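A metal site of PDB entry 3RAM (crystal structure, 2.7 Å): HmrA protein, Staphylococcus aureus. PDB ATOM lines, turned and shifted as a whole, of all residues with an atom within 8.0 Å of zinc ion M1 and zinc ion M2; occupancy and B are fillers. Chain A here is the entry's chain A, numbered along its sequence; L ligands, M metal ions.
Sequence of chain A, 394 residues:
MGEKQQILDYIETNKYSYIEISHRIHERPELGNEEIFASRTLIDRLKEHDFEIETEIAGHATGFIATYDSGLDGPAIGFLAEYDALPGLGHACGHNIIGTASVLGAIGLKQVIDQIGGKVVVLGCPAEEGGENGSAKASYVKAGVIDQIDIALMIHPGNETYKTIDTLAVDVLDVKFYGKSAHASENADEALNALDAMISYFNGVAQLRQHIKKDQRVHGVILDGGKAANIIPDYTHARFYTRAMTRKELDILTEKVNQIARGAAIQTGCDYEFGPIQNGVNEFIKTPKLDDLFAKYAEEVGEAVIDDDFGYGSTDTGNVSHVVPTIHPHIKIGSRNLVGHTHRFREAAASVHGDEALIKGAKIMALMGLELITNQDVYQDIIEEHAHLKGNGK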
ATOM      1  N   GLU A  82     -12.736  18.329 -34.698  1.00  0.00           N
ATOM      2  CA  GLU A  82     -12.436  19.408 -33.752  1.00  0.00           C
ATOM      3  C   GLU A  82     -11.007  19.194 -33.206  1.00  0.00           C
ATOM      4  O   GLU A  82     -10.531  18.055 -33.106  1.00  0.00           O
ATOM      5  CB  GLU A  82     -13.444  19.408 -32.593  1.00  0.00           C
ATOM      6  CG  GLU A  82     -14.913  19.700 -32.987  1.00  0.00           C
ATOM      7  CD  GLU A  82     -15.867  19.707 -31.792  1.00  0.00           C
ATOM      8  OE1 GLU A  82     -15.427  19.391 -30.665  1.00  0.00           O
ATOM      9  OE2 GLU A  82     -17.054  20.035 -31.986  1.00  0.00           O
ATOM     10  N   ASP A  84      -9.205  22.150 -30.987  1.00  0.00           N
ATOM     11  CA  ASP A  84      -8.766  23.290 -30.145  1.00  0.00           C
ATOM     12  C   ASP A  84      -8.673  22.931 -28.667  1.00  0.00           C
ATOM     13  O   ASP A  84      -9.499  22.186 -28.145  1.00  0.00           O
ATOM     14  CB  ASP A  84      -9.681  24.529 -30.329  1.00  0.00           C
ATOM     15  CG  ASP A  84     -11.146  24.280 -29.947  1.00  0.00           C
ATOM     16  OD1 ASP A  84     -11.699  23.236 -30.377  1.00  0.00           O
ATOM     17  OD2 ASP A  84     -11.756  25.132 -29.262  1.00  0.00           O
ATOM     18  N   ALA A  85      -7.643  23.459 -27.993  1.00  0.00           N
ATOM     19  CA  ALA A  85      -7.436  23.235 -26.553  1.00  0.00           C
ATOM     20  C   ALA A  85      -8.132  24.314 -25.731  1.00  0.00           C
ATOM     21  O   ALA A  85      -8.781  25.212 -26.295  1.00  0.00           O
ATOM     22  CB  ALA A  85      -5.947  23.198 -26.248  1.00  0.00           C
ATOM     23  N   LEU A  86      -7.994  24.221 -24.415  1.00  0.00           N
ATOM     24  CA  LEU A  86      -8.483  25.247 -23.468  1.00  0.00           C
ATOM     25  C   LEU A  86      -7.287  26.014 -22.856  1.00  0.00           C
ATOM     26  O   LEU A  86      -6.205  25.440 -22.706  1.00  0.00           O
ATOM     27  CB  LEU A  86      -9.360  24.596 -22.381  1.00  0.00           C
ATOM     28  CG  LEU A  86     -10.769  24.139 -22.814  1.00  0.00           C
ATOM     29  CD1 LEU A  86     -11.295  23.011 -21.924  1.00  0.00           C
ATOM     30  CD2 LEU A  86     -11.754  25.321 -22.874  1.00  0.00           C
ATOM     31  N   ALA A  92      -8.367  19.527 -22.003  1.00  0.00           N
ATOM     32  CA  ALA A  92      -9.230  19.028 -20.954  1.00  0.00           C
ATOM     33  C   ALA A  92     -10.681  18.788 -21.438  1.00  0.00           C
ATOM     34  O   ALA A  92     -11.554  18.509 -20.610  1.00  0.00           O
ATOM     35  CB  ALA A  92      -9.218  20.002 -19.756  1.00  0.00           C
ATOM     36  N   CYS A  93     -10.938  18.934 -22.746  1.00  0.00           N
ATOM     37  CA  CYS A  93     -12.197  18.471 -23.364  1.00  0.00           C
ATOM     38  C   CYS A  93     -11.977  17.326 -24.361  1.00  0.00           C
ATOM     39  O   CYS A  93     -12.931  16.849 -24.983  1.00  0.00           O
ATOM     40  CB  CYS A  93     -12.881  19.613 -24.097  1.00  0.00           C
ATOM     41  SG  CYS A  93     -14.685  19.554 -24.002  1.00  0.00           S
ATOM     42  N   GLY A  94     -10.722  16.895 -24.506  1.00  0.00           N
ATOM     43  CA  GLY A  94     -10.361  15.736 -25.329  1.00  0.00           C
ATOM     44  C   GLY A  94     -10.516  15.917 -26.825  1.00  0.00           C
ATOM     45  O   GLY A  94     -10.838  14.981 -27.529  1.00  0.00           O
ATOM     46  N   HIS A  95     -10.278  17.122 -27.318  1.00  0.00           N
ATOM     47  CA  HIS A  95     -10.471  17.434 -28.736  1.00  0.00           C
ATOM     48  C   HIS A  95      -9.399  16.836 -29.665  1.00  0.00           C
ATOM     49  O   HIS A  95      -9.599  16.753 -30.886  1.00  0.00           O
ATOM     50  CB  HIS A  95     -10.554  18.934 -28.908  1.00  0.00           C
ATOM     51  CG  HIS A  95     -11.869  19.497 -28.497  1.00  0.00           C
ATOM     52  ND1 HIS A  95     -12.270  20.775 -28.832  1.00  0.00           N
ATOM     53  CD2 HIS A  95     -12.907  18.947 -27.818  1.00  0.00           C
ATOM     54  CE1 HIS A  95     -13.476  20.995 -28.345  1.00  0.00           C
ATOM     55  NE2 HIS A  95     -13.889  19.901 -27.736  1.00  0.00           N
ATOM     56  N   ILE A  98     -11.263  13.859 -30.970  1.00  0.00           N
ATOM     57  CA  ILE A  98     -12.390  14.111 -31.861  1.00  0.00           C
ATOM     58  C   ILE A  98     -11.889  14.235 -33.303  1.00  0.00           C
ATOM     59  O   ILE A  98     -12.333  13.489 -34.179  1.00  0.00           O
ATOM     60  CB  ILE A  98     -13.212  15.360 -31.418  1.00  0.00           C
ATOM     61  CG1 ILE A  98     -13.708  15.170 -29.975  1.00  0.00           C
ATOM     62  CG2 ILE A  98     -14.382  15.594 -32.364  1.00  0.00           C
ATOM     63  CD1 ILE A  98     -14.568  16.296 -29.420  1.00  0.00           C
ATOM     64  N   GLU A 128     -14.349  25.485 -31.267  1.00  0.00           N
ATOM     65  CA  GLU A 128     -15.717  25.127 -30.766  1.00  0.00           C
ATOM     66  C   GLU A 128     -15.923  25.553 -29.332  1.00  0.00           C
ATOM     67  O   GLU A 128     -17.049  25.575 -28.870  1.00  0.00           O
ATOM     68  CB  GLU A 128     -16.076  23.633 -30.907  1.00  0.00           C
ATOM     69  CG  GLU A 128     -15.888  22.788 -29.649  1.00  0.00           C
ATOM     70  CD  GLU A 128     -17.127  22.563 -28.779  1.00  0.00           C
ATOM     71  OE1 GLU A 128     -16.960  22.302 -27.559  1.00  0.00           O
ATOM     72  OE2 GLU A 128     -18.255  22.599 -29.309  1.00  0.00           O
ATOM     73  N   GLU A 129     -14.833  25.858 -28.615  1.00  0.00           N
ATOM     74  CA  GLU A 129     -14.933  26.308 -27.240  1.00  0.00           C
ATOM     75  C   GLU A 129     -15.353  27.772 -27.208  1.00  0.00           C
ATOM     76  O   GLU A 129     -15.723  28.275 -26.155  1.00  0.00           O
ATOM     77  CB  GLU A 129     -13.609  26.093 -26.507  1.00  0.00           C
ATOM     78  CG  GLU A 129     -13.220  24.608 -26.331  1.00  0.00           C
ATOM     79  CD  GLU A 129     -14.135  23.850 -25.373  1.00  0.00           C
ATOM     80  OE1 GLU A 129     -13.953  22.627 -25.213  1.00  0.00           O
ATOM     81  OE2 GLU A 129     -15.032  24.479 -24.786  1.00  0.00           O
ATOM     82  N   GLY A 130     -15.329  28.435 -28.349  1.00  0.00           N
ATOM     83  CA  GLY A 130     -15.866  29.795 -28.470  1.00  0.00           C
ATOM     84  C   GLY A 130     -14.782  30.827 -28.337  1.00  0.00           C
ATOM     85  O   GLY A 130     -13.607  30.472 -28.292  1.00  0.00           O
ATOM     86  N   MET A 154     -19.895  12.615 -35.803  1.00  0.00           N
ATOM     87  CA  MET A 154     -18.939  13.087 -34.802  1.00  0.00           C
ATOM     88  C   MET A 154     -19.059  12.236 -33.533  1.00  0.00           C
ATOM     89  O   MET A 154     -20.109  11.659 -33.284  1.00  0.00           O
ATOM     90  CB  MET A 154     -19.309  14.507 -34.457  1.00  0.00           C
ATOM     91  CG  MET A 154     -18.330  15.215 -33.573  1.00  0.00           C
ATOM     92  SD  MET A 154     -19.215  16.771 -32.810  1.00  0.00           S
ATOM     93  CE  MET A 154     -17.961  17.043 -31.295  1.00  0.00           C
ATOM     94  N   ILE A 155     -17.984  12.148 -32.751  1.00  0.00           N
ATOM     95  CA  ILE A 155     -18.054  11.548 -31.414  1.00  0.00           C
ATOM     96  C   ILE A 155     -17.304  12.467 -30.441  1.00  0.00           C
ATOM     97  O   ILE A 155     -16.373  13.177 -30.848  1.00  0.00           O
ATOM     98  CB  ILE A 155     -17.503  10.095 -31.350  1.00  0.00           C
ATOM     99  CG1 ILE A 155     -15.999  10.043 -31.682  1.00  0.00           C
ATOM    100  CG2 ILE A 155     -18.314   9.170 -32.278  1.00  0.00           C
ATOM    101  CD1 ILE A 155     -15.050  10.351 -30.504  1.00  0.00           C
ATOM    102  N   HIS A 156     -17.743  12.499 -29.178  1.00  0.00           N
ATOM    103  CA  HIS A 156     -17.152  13.352 -28.160  1.00  0.00           C
ATOM    104  C   HIS A 156     -16.754  12.558 -26.904  1.00  0.00           C
ATOM    105  O   HIS A 156     -17.623  12.000 -26.229  1.00  0.00           O
ATOM    106  CB  HIS A 156     -18.096  14.514 -27.773  1.00  0.00           C
ATOM    107  CG  HIS A 156     -17.386  15.657 -27.108  1.00  0.00           C
ATOM    108  ND1 HIS A 156     -16.707  15.535 -25.918  1.00  0.00           N
ATOM    109  CD2 HIS A 156     -17.231  16.952 -27.494  1.00  0.00           C
ATOM    110  CE1 HIS A 156     -16.174  16.688 -25.593  1.00  0.00           C
ATOM    111  NE2 HIS A 156     -16.470  17.566 -26.528  1.00  0.00           N
ATOM    112  N   PRO A 157     -15.457  12.531 -26.551  1.00  0.00           N
ATOM    113  CA  PRO A 157     -15.083  11.759 -25.379  1.00  0.00           C
ATOM    114  C   PRO A 157     -15.862  12.212 -24.143  1.00  0.00           C
ATOM    115  O   PRO A 157     -16.109  13.401 -23.995  1.00  0.00           O
ATOM    116  CB  PRO A 157     -13.579  12.050 -25.215  1.00  0.00           C
ATOM    117  CG  PRO A 157     -13.265  13.171 -26.111  1.00  0.00           C
ATOM    118  CD  PRO A 157     -14.284  13.165 -27.191  1.00  0.00           C
ATOM    119  N   SER A 314     -23.646  22.658 -25.151  1.00  0.00           N
ATOM    120  CA  SER A 314     -23.619  24.001 -25.684  1.00  0.00           C
ATOM    121  C   SER A 314     -22.525  24.083 -26.740  1.00  0.00           C
ATOM    122  O   SER A 314     -21.414  24.554 -26.452  1.00  0.00           O
ATOM    123  CB  SER A 314     -23.374  24.995 -24.540  1.00  0.00           C
ATOM    124  OG  SER A 314     -23.835  26.277 -24.905  1.00  0.00           O
ATOM    125  N   THR A 315     -22.851  23.625 -27.946  1.00  0.00           N
ATOM    126  CA  THR A 315     -21.845  23.393 -28.995  1.00  0.00           C
ATOM    127  C   THR A 315     -22.354  23.886 -30.343  1.00  0.00           C
ATOM    128  O   THR A 315     -23.553  23.833 -30.614  1.00  0.00           O
ATOM    129  CB  THR A 315     -21.505  21.881 -29.088  1.00  0.00           C
ATOM    130  OG1 THR A 315     -20.516  21.670 -30.090  1.00  0.00           O
ATOM    131  CG2 THR A 315     -22.763  21.038 -29.407  1.00  0.00           C
ATOM    132  N   HIS A 328     -24.134  14.293 -31.910  1.00  0.00           N
ATOM    133  CA  HIS A 328     -23.112  14.763 -30.981  1.00  0.00           C
ATOM    134  C   HIS A 328     -23.183  13.847 -29.763  1.00  0.00           C
ATOM    135  O   HIS A 328     -23.690  14.239 -28.710  1.00  0.00           O
ATOM    136  CB  HIS A 328     -23.358  16.220 -30.618  1.00  0.00           C
ATOM    137  CG  HIS A 328     -22.382  16.784 -29.631  1.00  0.00           C
ATOM    138  ND1 HIS A 328     -22.729  17.055 -28.322  1.00  0.00           N
ATOM    139  CD2 HIS A 328     -21.088  17.165 -29.759  1.00  0.00           C
ATOM    140  CE1 HIS A 328     -21.679  17.572 -27.693  1.00  0.00           C
ATOM    141  NE2 HIS A 328     -20.669  17.641 -28.540  1.00  0.00           N
ATOM    142  N   HIS A 330     -21.394  10.742 -27.048  1.00  0.00           N
ATOM    143  CA  HIS A 330     -20.190  10.629 -26.269  1.00  0.00           C
ATOM    144  C   HIS A 330     -19.671   9.180 -26.224  1.00  0.00           C
ATOM    145  O   HIS A 330     -20.448   8.229 -26.299  1.00  0.00           O
ATOM    146  CB  HIS A 330     -20.489  11.148 -24.870  1.00  0.00           C
ATOM    147  CG  HIS A 330     -20.505  12.646 -24.767  1.00  0.00           C
ATOM    148  ND1 HIS A 330     -21.567  13.412 -25.225  1.00  0.00           N
ATOM    149  CD2 HIS A 330     -19.631  13.520 -24.216  1.00  0.00           C
ATOM    150  CE1 HIS A 330     -21.323  14.683 -24.972  1.00  0.00           C
ATOM    151  NE2 HIS A 330     -20.163  14.773 -24.360  1.00  0.00           N
ATOM    152  N   GLY A 340     -15.819  17.065 -17.643  1.00  0.00           N
ATOM    153  CA  GLY A 340     -15.144  17.800 -18.723  1.00  0.00           C
ATOM    154  C   GLY A 340     -14.466  19.067 -18.221  1.00  0.00           C
ATOM    155  O   GLY A 340     -14.863  19.613 -17.177  1.00  0.00           O
ATOM    156  N   HIS A 341     -13.462  19.511 -18.973  1.00  0.00           N
ATOM    157  CA  HIS A 341     -12.655  20.705 -18.657  1.00  0.00           C
ATOM    158  C   HIS A 341     -11.954  20.641 -17.268  1.00  0.00           C
ATOM    159  O   HIS A 341     -11.845  21.645 -16.570  1.00  0.00           O
ATOM    160  CB  HIS A 341     -13.511  21.979 -18.719  1.00  0.00           C
ATOM    161  CG  HIS A 341     -14.026  22.314 -20.079  1.00  0.00           C
ATOM    162  ND1 HIS A 341     -14.323  23.613 -20.450  1.00  0.00           N
ATOM    163  CD2 HIS A 341     -14.310  21.540 -21.152  1.00  0.00           C
ATOM    164  CE1 HIS A 341     -14.773  23.615 -21.690  1.00  0.00           C
ATOM    165  NE2 HIS A 341     -14.772  22.381 -22.144  1.00  0.00           N
ATOM    166  N   PHE A 345      -9.527  15.089 -16.921  1.00  0.00           N
ATOM    167  CA  PHE A 345     -10.080  14.798 -18.242  1.00  0.00           C
ATOM    168  C   PHE A 345      -8.988  14.837 -19.300  1.00  0.00           C
ATOM    169  O   PHE A 345      -8.917  13.950 -20.147  1.00  0.00           O
ATOM    170  CB  PHE A 345     -11.205  15.772 -18.579  1.00  0.00           C
ATOM    171  CG  PHE A 345     -12.175  15.259 -19.631  1.00  0.00           C
ATOM    172  CD1 PHE A 345     -13.359  14.636 -19.252  1.00  0.00           C
ATOM    173  CD2 PHE A 345     -11.909  15.412 -20.981  1.00  0.00           C
ATOM    174  CE1 PHE A 345     -14.250  14.174 -20.198  1.00  0.00           C
ATOM    175  CE2 PHE A 345     -12.787  14.944 -21.922  1.00  0.00           C
ATOM    176  CZ  PHE A 345     -13.960  14.338 -21.531  1.00  0.00           C
HETATM  177  C1  LIG L   1     -18.589  23.028 -24.517  1.00  0.00           C
HETATM  178  O1  LIG L   1     -18.809  24.197 -25.283  1.00  0.00           O
HETATM  179  C2  LIG L   1     -18.921  21.767 -25.326  1.00  0.00           C
HETATM  180  O2  LIG L   1     -17.721  21.057 -25.556  1.00  0.00           O
HETATM  181  C3  LIG L   1     -19.996  20.940 -24.582  1.00  0.00           C
HETATM  182  O3  LIG L   1     -20.445  19.755 -25.254  1.00  0.00           O
HETATM  183 ZN    ZN M   1     -15.440  21.777 -24.097  1.00  0.00          ZN
HETATM  184 ZN    ZN M   2     -15.652  19.542 -26.561  1.00  0.00          ZN
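A ring nitrogen (ND1) of His 95 lies within hydrogen-bond range of the side-chain carboxylate (OD1) of Asp 84. N of Glu 129 sits at hydrogen-bond distance from OD2 of Asp 84, 3.2 Å away. The side-chain hydroxyl (OG1) of Thr 315 lies within hydrogen-bond range of the side-chain carboxylate (OE2) of Glu 128, 2.6 Å away. The backbone NH (N) of His 341 lies within hydrogen-bond range of the backbone carbonyl oxygen (O) of Ala 92. NE2 of His 95 lies close to OE1 of Glu 82 (3.3 Å). OD2 of Asp 84 lies within hydrogen-bond range of N of Glu 128 (3.3 Å).
Residues that only touch zinc ion M1: Glu 128 (3.8 Å). Four residues have an atom within 4 Å of zinc ion M1: Cys 93, Glu 128, Glu 129 and His 341. The nearest printed residue that does not touch zinc ion M1 is His 95 (4.4 Å).
Residues that only touch zinc ion M2: Glu 128 (3.2 Å). Within 4 Å of zinc ion M2: Cys 93, His 95, Glu 128, Glu 129 and His 156. The nearest printed residue that does not touch zinc ion M2 is Glu 82 (4.1 Å).
Zinc ion M1 is bound by the side-chain carboxylate (OE1) of Glu 129 (2.0 Å), a ring nitrogen (NE2) of His 341 (2.2 Å) and the side-chain sulfur (SG) of Cys 93 (2.3 Å). Slightly farther from zinc ion M1 lies an oxygen (O2) of the ligand (2.8 Å). Slightly farther from zinc ion M1 lies the side-chain carboxylate (OE2) of Glu 129 (2.8 Å).
Zinc ion M2 is bound by a ring nitrogen (NE2) of His 156 (2.1 Å), a ring nitrogen (NE2) of His 95 (2.1 Å) and the side-chain sulfur of Cys 93 (2.7 Å). Zinc ion M2 has three donor atoms within binding distance. Slightly farther from zinc ion M2 lies an oxygen (O2) of the ligand (2.8 Å).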
